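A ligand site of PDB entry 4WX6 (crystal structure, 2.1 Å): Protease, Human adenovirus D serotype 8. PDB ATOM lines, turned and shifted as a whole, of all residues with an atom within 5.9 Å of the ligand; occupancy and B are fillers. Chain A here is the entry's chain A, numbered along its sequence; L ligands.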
ATOM      1  N   SER A   1      -2.072 -17.030 -12.354  1.00  0.00           N
ATOM      2  CA  SER A   1      -0.772 -17.766 -12.108  1.00  0.00           C
ATOM      3  C   SER A   1      -0.482 -17.914 -10.612  1.00  0.00           C
ATOM      4  O   SER A   1      -0.083 -16.961  -9.921  1.00  0.00           O
ATOM      5  CB  SER A   1       0.413 -17.097 -12.856  1.00  0.00           C
ATOM      6  OG  SER A   1       1.683 -17.628 -12.459  1.00  0.00           O
ATOM      7  N   GLY A   2      -0.672 -19.120 -10.100  1.00  0.00           N
ATOM      8  CA  GLY A   2      -0.440 -19.380  -8.684  1.00  0.00           C
ATOM      9  C   GLY A   2      -1.482 -18.843  -7.723  1.00  0.00           C
ATOM     10  O   GLY A   2      -2.542 -18.293  -8.100  1.00  0.00           O
ATOM     11  N   SER A   3      -1.148 -19.035  -6.454  1.00  0.00           N
ATOM     12  CA  SER A   3      -2.024 -18.749  -5.355  1.00  0.00           C
ATOM     13  C   SER A   3      -1.492 -17.487  -4.732  1.00  0.00           C
ATOM     14  O   SER A   3      -0.269 -17.247  -4.740  1.00  0.00           O
ATOM     15  CB  SER A   3      -1.980 -19.902  -4.344  1.00  0.00           C
ATOM     16  OG  SER A   3      -2.022 -21.189  -4.969  1.00  0.00           O
ATOM     17  N   SER A   4      -2.383 -16.663  -4.220  1.00  0.00           N
ATOM     18  CA  SER A   4      -1.974 -15.366  -3.694  1.00  0.00           C
ATOM     19  C   SER A   4      -1.842 -15.512  -2.197  1.00  0.00           C
ATOM     20  O   SER A   4      -2.314 -16.522  -1.629  1.00  0.00           O
ATOM     21  CB  SER A   4      -2.986 -14.270  -4.053  1.00  0.00           C
ATOM     22  OG  SER A   4      -4.153 -14.494  -3.282  1.00  0.00           O
ATOM     23  N   GLU A   5      -1.222 -14.517  -1.539  1.00  0.00           N
ATOM     24  CA  GLU A   5      -1.082 -14.594  -0.081  1.00  0.00           C
ATOM     25  C   GLU A   5      -2.404 -14.901   0.651  1.00  0.00           C
ATOM     26  O   GLU A   5      -2.416 -15.743   1.557  1.00  0.00           O
ATOM     27  CB  GLU A   5      -0.333 -13.390   0.506  1.00  0.00           C
ATOM     28  CG  GLU A   5      -0.930 -12.010   0.300  1.00  0.00           C
ATOM     29  CD  GLU A   5      -0.235 -10.968   1.177  1.00  0.00           C
ATOM     30  OE1 GLU A   5       0.658 -10.264   0.660  1.00  0.00           O
ATOM     31  OE2 GLU A   5      -0.553 -10.854   2.387  1.00  0.00           O
ATOM     32  N   GLN A   6      -3.497 -14.236   0.254  1.00  0.00           N
ATOM     33  CA  GLN A   6      -4.837 -14.430   0.892  1.00  0.00           C
ATOM     34  C   GLN A   6      -5.320 -15.855   0.748  1.00  0.00           C
ATOM     35  O   GLN A   6      -5.755 -16.471   1.713  1.00  0.00           O
ATOM     36  CB  GLN A   6      -5.891 -13.511   0.274  1.00  0.00           C
ATOM     37  CG  GLN A   6      -5.469 -12.059   0.137  1.00  0.00           C
ATOM     38  CD  GLN A   6      -4.828 -11.781  -1.206  1.00  0.00           C
ATOM     39  OE1 GLN A   6      -5.414 -12.086  -2.256  1.00  0.00           O
ATOM     40  NE2 GLN A   6      -3.622 -11.204  -1.192  1.00  0.00           N
ATOM     41  N   THR A  24       2.266 -14.867   6.087  1.00  0.00           N
ATOM     42  CA  THR A  24       2.905 -15.024   4.794  1.00  0.00           C
ATOM     43  C   THR A  24       3.900 -13.910   4.610  1.00  0.00           C
ATOM     44  O   THR A  24       3.554 -12.757   4.805  1.00  0.00           O
ATOM     45  CB  THR A  24       1.906 -15.071   3.615  1.00  0.00           C
ATOM     46  OG1 THR A  24       1.727 -13.749   3.105  1.00  0.00           O
ATOM     47  CG2 THR A  24       0.524 -15.637   4.011  1.00  0.00           C
ATOM     48  N   HIS A  25       5.143 -14.283   4.251  1.00  0.00           N
ATOM     49  CA  HIS A  25       6.267 -13.342   4.145  1.00  0.00           C
ATOM     50  C   HIS A  25       6.913 -13.295   2.768  1.00  0.00           C
ATOM     51  O   HIS A  25       6.943 -14.287   2.084  1.00  0.00           O
ATOM     52  CB  HIS A  25       7.332 -13.639   5.193  1.00  0.00           C
ATOM     53  CG  HIS A  25       6.863 -13.421   6.591  1.00  0.00           C
ATOM     54  ND1 HIS A  25       5.936 -14.256   7.190  1.00  0.00           N
ATOM     55  CD2 HIS A  25       7.134 -12.434   7.480  1.00  0.00           C
ATOM     56  CE1 HIS A  25       5.689 -13.812   8.414  1.00  0.00           C
ATOM     57  NE2 HIS A  25       6.401 -12.713   8.614  1.00  0.00           N
ATOM     58  N   ASP A  26       7.416 -12.128   2.379  1.00  0.00           N
ATOM     59  CA  ASP A  26       8.288 -12.020   1.235  1.00  0.00           C
ATOM     60  C   ASP A  26       9.530 -12.883   1.581  1.00  0.00           C
ATOM     61  O   ASP A  26       9.551 -13.584   2.608  1.00  0.00           O
ATOM     62  CB  ASP A  26       8.681 -10.526   1.012  1.00  0.00           C
ATOM     63  CG  ASP A  26       9.540  -9.957   2.151  1.00  0.00           C
ATOM     64  OD1 ASP A  26       9.542 -10.521   3.260  1.00  0.00           O
ATOM     65  OD2 ASP A  26      10.225  -8.931   1.931  1.00  0.00           O
ATOM     66  N   LYS A  27      10.567 -12.788   0.749  1.00  0.00           N
ATOM     67  CA  LYS A  27      11.802 -13.527   1.031  1.00  0.00           C
ATOM     68  C   LYS A  27      12.533 -13.180   2.345  1.00  0.00           C
ATOM     69  O   LYS A  27      13.590 -13.716   2.597  1.00  0.00           O
ATOM     70  CB  LYS A  27      12.766 -13.366  -0.145  1.00  0.00           C
ATOM     71  CG  LYS A  27      13.286 -11.930  -0.273  1.00  0.00           C
ATOM     72  CD  LYS A  27      14.358 -11.926  -1.358  1.00  0.00           C
ATOM     73  CE  LYS A  27      14.979 -10.559  -1.608  1.00  0.00           C
ATOM     74  NZ  LYS A  27      15.664 -10.630  -2.931  1.00  0.00           N
ATOM     75  N   ILE A  42       4.914 -19.316   5.613  1.00  0.00           N
ATOM     76  CA  ILE A  42       5.012 -19.356   4.158  1.00  0.00           C
ATOM     77  C   ILE A  42       5.824 -18.129   3.751  1.00  0.00           C
ATOM     78  O   ILE A  42       5.561 -17.011   4.177  1.00  0.00           O
ATOM     79  CB  ILE A  42       3.623 -19.396   3.482  1.00  0.00           C
ATOM     80  CG1 ILE A  42       3.006 -20.806   3.642  1.00  0.00           C
ATOM     81  CG2 ILE A  42       3.716 -18.981   2.022  1.00  0.00           C
ATOM     82  CD1 ILE A  42       1.577 -20.934   3.117  1.00  0.00           C
ATOM     83  N   ASN A  44       7.826 -16.300   0.485  1.00  0.00           N
ATOM     84  CA  ASN A  44       8.017 -16.258  -0.948  1.00  0.00           C
ATOM     85  C   ASN A  44       9.499 -16.269  -1.243  1.00  0.00           C
ATOM     86  O   ASN A  44      10.271 -15.692  -0.489  1.00  0.00           O
ATOM     87  CB  ASN A  44       7.419 -14.981  -1.537  1.00  0.00           C
ATOM     88  CG  ASN A  44       7.022 -15.154  -3.000  1.00  0.00           C
ATOM     89  OD1 ASN A  44       5.946 -15.680  -3.291  1.00  0.00           O
ATOM     90  ND2 ASN A  44       7.872 -14.709  -3.906  1.00  0.00           N
ATOM     91  N   THR A  45       9.901 -16.862  -2.351  1.00  0.00           N
ATOM     92  CA  THR A  45      11.296 -16.816  -2.725  1.00  0.00           C
ATOM     93  C   THR A  45      11.759 -15.429  -3.047  1.00  0.00           C
ATOM     94  O   THR A  45      12.940 -15.128  -2.900  1.00  0.00           O
ATOM     95  CB  THR A  45      11.629 -17.659  -3.956  1.00  0.00           C
ATOM     96  OG1 THR A  45      10.775 -17.272  -5.057  1.00  0.00           O
ATOM     97  CG2 THR A  45      11.515 -19.169  -3.646  1.00  0.00           C
ATOM     98  N   ALA A  46      10.854 -14.599  -3.555  1.00  0.00           N
ATOM     99  CA  ALA A  46      11.228 -13.247  -3.973  1.00  0.00           C
ATOM    100  C   ALA A  46      10.807 -12.179  -2.967  1.00  0.00           C
ATOM    101  O   ALA A  46       9.952 -12.426  -2.091  1.00  0.00           O
ATOM    102  CB  ALA A  46      10.699 -12.938  -5.360  1.00  0.00           C
ATOM    103  N   GLY A  47      11.429 -11.013  -3.057  1.00  0.00           N
ATOM    104  CA  GLY A  47      11.019  -9.850  -2.275  1.00  0.00           C
ATOM    105  C   GLY A  47       9.702  -9.271  -2.774  1.00  0.00           C
ATOM    106  O   GLY A  47       9.477  -9.211  -3.985  1.00  0.00           O
ATOM    107  N   ARG A  48       8.864  -8.808  -1.832  1.00  0.00           N
ATOM    108  CA  ARG A  48       7.480  -8.401  -2.094  1.00  0.00           C
ATOM    109  C   ARG A  48       7.295  -7.584  -3.365  1.00  0.00           C
ATOM    110  O   ARG A  48       6.223  -7.588  -3.960  1.00  0.00           O
ATOM    111  CB  ARG A  48       6.939  -7.600  -0.905  1.00  0.00           C
ATOM    112  CG  ARG A  48       5.436  -7.758  -0.695  1.00  0.00           C
ATOM    113  CD  ARG A  48       5.075  -7.236   0.688  1.00  0.00           C
ATOM    114  NE  ARG A  48       4.999  -8.353   1.625  1.00  0.00           N
ATOM    115  CZ  ARG A  48       3.847  -8.901   2.010  1.00  0.00           C
ATOM    116  NH1 ARG A  48       3.842  -9.927   2.864  1.00  0.00           N
ATOM    117  NH2 ARG A  48       2.692  -8.452   1.521  1.00  0.00           N
ATOM    118  N   GLU A  49       8.371  -6.884  -3.736  1.00  0.00           N
ATOM    119  CA  GLU A  49       8.420  -5.828  -4.727  1.00  0.00           C
ATOM    120  C   GLU A  49       8.753  -6.347  -6.116  1.00  0.00           C
ATOM    121  O   GLU A  49       9.105  -5.600  -7.047  1.00  0.00           O
ATOM    122  CB  GLU A  49       9.485  -4.804  -4.296  1.00  0.00           C
ATOM    123  CG  GLU A  49      10.945  -5.285  -4.420  1.00  0.00           C
ATOM    124  CD  GLU A  49      11.392  -6.275  -3.316  1.00  0.00           C
ATOM    125  OE1 GLU A  49      11.668  -7.433  -3.681  1.00  0.00           O
ATOM    126  OE2 GLU A  49      11.470  -5.887  -2.125  1.00  0.00           O
ATOM    127  N   THR A  50       8.691  -7.656  -6.254  1.00  0.00           N
ATOM    128  CA  THR A  50       8.828  -8.258  -7.545  1.00  0.00           C
ATOM    129  C   THR A  50       7.420  -8.574  -7.967  1.00  0.00           C
ATOM    130  O   THR A  50       7.166  -8.859  -9.146  1.00  0.00           O
ATOM    131  CB  THR A  50       9.501  -9.628  -7.432  1.00  0.00           C
ATOM    132  OG1 THR A  50       8.712 -10.456  -6.544  1.00  0.00           O
ATOM    133  CG2 THR A  50      10.938  -9.495  -6.908  1.00  0.00           C
ATOM    134  N   GLY A  51       6.503  -8.563  -6.998  1.00  0.00           N
ATOM    135  CA  GLY A  51       5.186  -9.143  -7.199  1.00  0.00           C
ATOM    136  C   GLY A  51       5.089 -10.485  -6.510  1.00  0.00           C
ATOM    137  O   GLY A  51       4.005 -10.868  -6.064  1.00  0.00           O
ATOM    138  N   GLY A  52       6.199 -11.238  -6.467  1.00  0.00           N
ATOM    139  CA  GLY A  52       6.247 -12.542  -5.785  1.00  0.00           C
ATOM    140  C   GLY A  52       6.299 -13.660  -6.796  1.00  0.00           C
ATOM    141  O   GLY A  52       5.530 -13.637  -7.756  1.00  0.00           O
ATOM    142  N   VAL A  53       7.159 -14.656  -6.519  1.00  0.00           N
ATOM    143  CA  VAL A  53       7.616 -15.701  -7.508  1.00  0.00           C
ATOM    144  C   VAL A  53       7.345 -17.139  -7.117  1.00  0.00           C
ATOM    145  O   VAL A  53       6.613 -17.793  -7.790  1.00  0.00           O
ATOM    146  CB  VAL A  53       9.110 -15.544  -7.861  1.00  0.00           C
ATOM    147  CG1 VAL A  53       9.683 -16.830  -8.516  1.00  0.00           C
ATOM    148  CG2 VAL A  53       9.273 -14.312  -8.758  1.00  0.00           C
ATOM    149  N   HIS A  54       7.885 -17.637  -6.010  1.00  0.00           N
ATOM    150  CA  HIS A  54       7.636 -19.071  -5.695  1.00  0.00           C
ATOM    151  C   HIS A  54       7.333 -19.214  -4.244  1.00  0.00           C
ATOM    152  O   HIS A  54       7.842 -18.459  -3.468  1.00  0.00           O
ATOM    153  CB  HIS A  54       8.894 -19.842  -6.116  1.00  0.00           C
ATOM    154  CG  HIS A  54       8.955 -21.274  -5.674  1.00  0.00           C
ATOM    155  ND1 HIS A  54       7.928 -22.174  -5.867  1.00  0.00           N
ATOM    156  CD2 HIS A  54      10.026 -22.009  -5.250  1.00  0.00           C
ATOM    157  CE1 HIS A  54       8.336 -23.381  -5.496  1.00  0.00           C
ATOM    158  NE2 HIS A  54       9.607 -23.311  -5.143  1.00  0.00           N
ATOM    159  N   TRP A  55       6.488 -20.161  -3.849  1.00  0.00           N
ATOM    160  CA  TRP A  55       6.130 -20.231  -2.437  1.00  0.00           C
ATOM    161  C   TRP A  55       6.979 -21.281  -1.747  1.00  0.00           C
ATOM    162  O   TRP A  55       7.225 -22.317  -2.330  1.00  0.00           O
ATOM    163  CB  TRP A  55       4.632 -20.565  -2.262  1.00  0.00           C
ATOM    164  CG  TRP A  55       3.676 -19.430  -2.630  1.00  0.00           C
ATOM    165  CD1 TRP A  55       2.674 -19.468  -3.552  1.00  0.00           C
ATOM    166  CD2 TRP A  55       3.632 -18.099  -2.057  1.00  0.00           C
ATOM    167  NE1 TRP A  55       2.018 -18.254  -3.598  1.00  0.00           N
ATOM    168  CE2 TRP A  55       2.588 -17.398  -2.692  1.00  0.00           C
ATOM    169  CE3 TRP A  55       4.385 -17.442  -1.066  1.00  0.00           C
ATOM    170  CZ2 TRP A  55       2.270 -16.077  -2.368  1.00  0.00           C
ATOM    171  CZ3 TRP A  55       4.054 -16.123  -0.754  1.00  0.00           C
ATOM    172  CH2 TRP A  55       3.008 -15.459  -1.406  1.00  0.00           C
ATOM    173  N   PHE A  73       9.459 -28.546  -5.104  1.00  0.00           N
ATOM    174  CA  PHE A  73      10.303 -29.244  -6.090  1.00  0.00           C
ATOM    175  C   PHE A  73      11.499 -30.064  -5.462  1.00  0.00           C
ATOM    176  O   PHE A  73      12.267 -30.724  -6.211  1.00  0.00           O
ATOM    177  CB  PHE A  73      10.892 -28.266  -7.153  1.00  0.00           C
ATOM    178  CG  PHE A  73       9.883 -27.461  -7.980  1.00  0.00           C
ATOM    179  CD1 PHE A  73       8.925 -28.077  -8.774  1.00  0.00           C
ATOM    180  CD2 PHE A  73      10.004 -26.073  -8.063  1.00  0.00           C
ATOM    181  CE1 PHE A  73       8.073 -27.321  -9.582  1.00  0.00           C
ATOM    182  CE2 PHE A  73       9.148 -25.305  -8.844  1.00  0.00           C
ATOM    183  CZ  PHE A  73       8.177 -25.932  -9.614  1.00  0.00           C
ATOM    184  N   TYR A  84      15.994 -18.877  -8.154  1.00  0.00           N
ATOM    185  CA  TYR A  84      15.040 -17.936  -7.535  1.00  0.00           C
ATOM    186  C   TYR A  84      15.655 -16.761  -6.833  1.00  0.00           C
ATOM    187  O   TYR A  84      14.968 -16.012  -6.111  1.00  0.00           O
ATOM    188  CB  TYR A  84      14.192 -18.726  -6.540  1.00  0.00           C
ATOM    189  CG  TYR A  84      13.291 -19.723  -7.212  1.00  0.00           C
ATOM    190  CD1 TYR A  84      12.288 -19.281  -8.094  1.00  0.00           C
ATOM    191  CD2 TYR A  84      13.359 -21.094  -6.925  1.00  0.00           C
ATOM    192  CE1 TYR A  84      11.438 -20.175  -8.693  1.00  0.00           C
ATOM    193  CE2 TYR A  84      12.504 -22.001  -7.541  1.00  0.00           C
ATOM    194  CZ  TYR A  84      11.531 -21.520  -8.446  1.00  0.00           C
ATOM    195  OH  TYR A  84      10.612 -22.372  -9.072  1.00  0.00           O
ATOM    196  N   GLN A 115       5.714 -31.532  -7.321  1.00  0.00           N
ATOM    197  CA  GLN A 115       5.174 -30.692  -8.343  1.00  0.00           C
ATOM    198  C   GLN A 115       5.672 -31.112  -9.729  1.00  0.00           C
ATOM    199  O   GLN A 115       6.765 -31.679  -9.853  1.00  0.00           O
ATOM    200  CB  GLN A 115       5.607 -29.256  -8.002  1.00  0.00           C
ATOM    201  CG  GLN A 115       4.910 -28.151  -8.805  1.00  0.00           C
ATOM    202  CD  GLN A 115       4.890 -26.805  -8.081  1.00  0.00           C
ATOM    203  OE1 GLN A 115       4.940 -26.779  -6.841  1.00  0.00           O
ATOM    204  NE2 GLN A 115       4.824 -25.689  -8.840  1.00  0.00           N
ATOM    205  N   PRO A 117       6.930 -29.681 -13.416  1.00  0.00           N
ATOM    206  CA  PRO A 117       7.802 -28.552 -13.785  1.00  0.00           C
ATOM    207  C   PRO A 117       7.043 -27.260 -14.084  1.00  0.00           C
ATOM    208  O   PRO A 117       7.554 -26.142 -13.841  1.00  0.00           O
ATOM    209  CB  PRO A 117       8.513 -29.020 -15.102  1.00  0.00           C
ATOM    210  CG  PRO A 117       7.848 -30.303 -15.493  1.00  0.00           C
ATOM    211  CD  PRO A 117       6.999 -30.822 -14.338  1.00  0.00           C
ATOM    212  N   SER A 119       3.606 -26.698 -13.487  1.00  0.00           N
ATOM    213  CA  SER A 119       2.543 -26.438 -12.532  1.00  0.00           C
ATOM    214  C   SER A 119       2.792 -25.127 -11.716  1.00  0.00           C
ATOM    215  O   SER A 119       3.910 -24.532 -11.722  1.00  0.00           O
ATOM    216  CB  SER A 119       2.345 -27.675 -11.649  1.00  0.00           C
ATOM    217  OG  SER A 119       1.287 -27.497 -10.703  1.00  0.00           O
ATOM    218  N   ALA A 120       1.702 -24.635 -11.113  1.00  0.00           N
ATOM    219  CA  ALA A 120       1.771 -23.450 -10.279  1.00  0.00           C
ATOM    220  C   ALA A 120       1.027 -23.708  -8.957  1.00  0.00           C
ATOM    221  O   ALA A 120       0.695 -22.776  -8.211  1.00  0.00           O
ATOM    222  CB  ALA A 120       1.243 -22.229 -11.053  1.00  0.00           C
ATOM    223  N   ALA A 121       0.795 -24.993  -8.669  1.00  0.00           N
ATOM    224  CA  ALA A 121       0.252 -25.453  -7.402  1.00  0.00           C
ATOM    225  C   ALA A 121       1.277 -25.306  -6.250  1.00  0.00           C
ATOM    226  O   ALA A 121       1.165 -25.972  -5.222  1.00  0.00           O
ATOM    227  CB  ALA A 121      -0.258 -26.908  -7.537  1.00  0.00           C
ATOM    228  N   CYS A 122       2.256 -24.398  -6.415  1.00  0.00           N
ATOM    229  CA  CYS A 122       3.341 -24.251  -5.430  1.00  0.00           C
ATOM    230  C   CYS A 122       2.906 -23.875  -3.984  1.00  0.00           C
ATOM    231  O   CYS A 122       3.420 -24.425  -3.044  1.00  0.00           O
ATOM    232  CB  CYS A 122       4.472 -23.362  -5.961  1.00  0.00           C
ATOM    233  SG  CYS A 122       3.926 -21.674  -6.300  1.00  0.00           S
ATOM    234  N   GLY A 123       1.933 -22.990  -3.814  1.00  0.00           N
ATOM    235  CA  GLY A 123       1.381 -22.748  -2.459  1.00  0.00           C
ATOM    236  C   GLY A 123       0.489 -23.866  -1.933  1.00  0.00           C
ATOM    237  O   GLY A 123       0.622 -24.330  -0.794  1.00  0.00           O
ATOM    238  N   MET A 201       2.388 -22.808 -16.557  1.00  0.00           N
ATOM    239  CA  MET A 201       3.506 -22.007 -17.084  1.00  0.00           C
ATOM    240  C   MET A 201       3.679 -22.033 -18.623  1.00  0.00           C
ATOM    241  O   MET A 201       4.390 -21.198 -19.196  1.00  0.00           O
ATOM    242  CB  MET A 201       4.821 -22.308 -16.330  1.00  0.00           C
ATOM    243  CG  MET A 201       4.639 -22.403 -14.830  1.00  0.00           C
ATOM    244  SD  MET A 201       3.933 -20.964 -13.973  1.00  0.00           S
ATOM    245  CE  MET A 201       4.956 -19.647 -14.674  1.00  0.00           C
HETATM  246  C1  LIG L   1       4.997 -12.126  -0.729  1.00  0.00           C
HETATM  247  C2  LIG L   1       5.341 -11.774  -2.021  1.00  0.00           C
HETATM  248  C3  LIG L   1       4.361 -11.398  -2.960  1.00  0.00           C
HETATM  249  C4  LIG L   1       1.387 -14.191  -5.561  1.00  0.00           C
HETATM  250  C5  LIG L   1       2.640 -15.012  -5.755  1.00  0.00           C
HETATM  251  C6  LIG L   1       0.668 -13.943  -6.947  1.00  0.00           C
HETATM  252  C7  LIG L   1       0.085 -15.209  -7.684  1.00  0.00           C
HETATM  253  C8  LIG L   1      -0.563 -12.989  -6.817  1.00  0.00           C
HETATM  254  C9  LIG L   1       1.778 -13.305  -7.856  1.00  0.00           C
HETATM  255  C10 LIG L   1       3.553 -17.158  -6.236  1.00  0.00           C
HETATM  256  C11 LIG L   1       3.026 -18.394  -6.868  1.00  0.00           C
HETATM  257  C12 LIG L   1       3.419 -20.212  -8.503  1.00  0.00           C
HETATM  258  C13 LIG L   1       4.400 -21.279  -7.986  1.00  0.00           C
HETATM  259  C14 LIG L   1       5.914 -21.016  -8.139  1.00  0.00           C
HETATM  260  C15 LIG L   1       5.813 -21.021 -10.813  1.00  0.00           C
HETATM  261  C16 LIG L   1       3.005 -11.379  -2.597  1.00  0.00           C
HETATM  262  C17 LIG L   1       2.659 -11.747  -1.309  1.00  0.00           C
HETATM  263  C18 LIG L   1       3.655 -12.100  -0.401  1.00  0.00           C
HETATM  264 CL1  LIG L   1       3.221 -12.557   1.186  1.00  0.00          CL
HETATM  265 CL2  LIG L   1       7.046 -11.812  -2.407  1.00  0.00          CL
HETATM  266  C19 LIG L   1       1.872 -11.020  -3.581  1.00  0.00           C
HETATM  267  C20 LIG L   1       1.323 -12.370  -3.983  1.00  0.00           C
HETATM  268  N1  LIG L   1       0.794 -10.224  -2.984  1.00  0.00           N
HETATM  269  O1  LIG L   1       0.480 -12.948  -3.295  1.00  0.00           O
HETATM  270  N2  LIG L   1       1.857 -12.908  -5.098  1.00  0.00           N
HETATM  271  N3  LIG L   1       2.409 -16.307  -5.986  1.00  0.00           N
HETATM  272  O2  LIG L   1       3.754 -14.480  -5.746  1.00  0.00           O
HETATM  273  N4  LIG L   1       3.812 -18.970  -7.847  1.00  0.00           N
HETATM  274  O3  LIG L   1       1.947 -18.806  -6.432  1.00  0.00           O
HETATM  275  S1  LIG L   1       6.694 -21.841  -9.462  1.00  0.00           S
HETATM  276  O4  LIG L   1       6.210 -23.233  -9.303  1.00  0.00           O
HETATM  277  O5  LIG L   1       8.124 -21.544  -9.609  1.00  0.00           O
HETATM  278  C21 LIG L   1       0.085  -9.330  -3.918  1.00  0.00           C
HETATM  279  C22 LIG L   1      -0.619  -8.222  -3.075  1.00  0.00           C
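SG of Cys 122 is covalently linked to C13 of the ligand (1.8 Å). An oxygen (O5) of the ligand lies within hydrogen-bond range of the side-chain hydroxyl (OH) of Tyr 84, at 2.7 Å. NE2 of Gln 115 lies within hydrogen-bond range of O4 of the ligand (2.9 Å). The indole nitrogen of Trp 55 lies within hydrogen-bond range of an oxygen (O3) of the ligand (2.9 Å). An oxygen (O1) of the ligand is in hydrogen-bond range of the backbone NH (N) of Glu 5. The side-chain carboxylate (OE1) of Glu 5 is in salt-bridge range of a nitrogen (N1) of the ligand (3.6 Å). N of Val 53 lies within hydrogen-bond range of O2 of the ligand (3.5 Å). O of Val 53 lies within hydrogen-bond range of N4 of the ligand (3.0 Å). N of Ser 3 sits at hydrogen-bond distance from O3 of the ligand. A nitrogen (N3) of the ligand is in hydrogen-bond range of the backbone carbonyl oxygen of Ser 3 (3.1 Å). The backbone carbonyl oxygen (O) of Gly 51 is in hydrogen-bond range of a nitrogen (N2) of the ligand, 3.1 Å away.
The side-chain amide nitrogen of Gln 115 lies within hydrogen-bond range of the backbone carbonyl oxygen of Ser 119 (3.2 Å). The indole nitrogen (NE1) of Trp 55 sits at hydrogen-bond distance from the backbone carbonyl oxygen (O) of Ser 3 (2.7 Å). The side-chain amide nitrogen (ND2) of Asn 44 sits close to the backbone NH (N) of Ala 46 (3.0 Å). N of Val 53 lies close to ND2 of Asn 44 (2.7 Å). The backbone carbonyl oxygen of His 54 sits close to the side-chain amide oxygen of Asn 44. The backbone carbonyl oxygen (O) of His 25 lies within hydrogen-bond range of the backbone NH (N) of Asn 44 (2.7 Å). The side-chain hydroxyl (OG) of Ser 119 is in hydrogen-bond range of the backbone NH (N) of Ala 121, 3.3 Å away. The side-chain hydroxyl (OG1) of Thr 50 sits at hydrogen-bond distance from the backbone carbonyl oxygen (O) of Gly 47 (2.9 Å).
O of Gly 52 sits close to O2 of the ligand, 2.8 Å away. Merely in contact with the ligand: Thr 24 (2.7 Å), Ser 1 (2.8 Å), Ala 46 (3.0 Å), Arg 48 (3.2 Å), His 54 (3.2 Å), Asn 44 (3.3 Å), Gly 2 (3.3 Å), Phe 73 (3.4 Å), Ser 4 (3.5 Å), Ser 119 (3.6 Å), Met 201 (3.7 Å), Gly 47 (3.7 Å), Ala 120 (3.8 Å) and Asp 26 (3.8 Å). 23 residues have an atom within 4 Å of the ligand: Ser 1, Gly 2, Ser 3, Ser 4, Glu 5, Thr 24, Asp 26, Asn 44, Ala 46, Gly 47, Arg 48, Gly 51, Gly 52, Val 53, His 54, Trp 55, Phe 73, Tyr 84, Gln 115, Ser 119, Ala 120, Cys 122 and Met 201. The nearest printed residue that does not touch the ligand is His 25 (4.01 Å).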
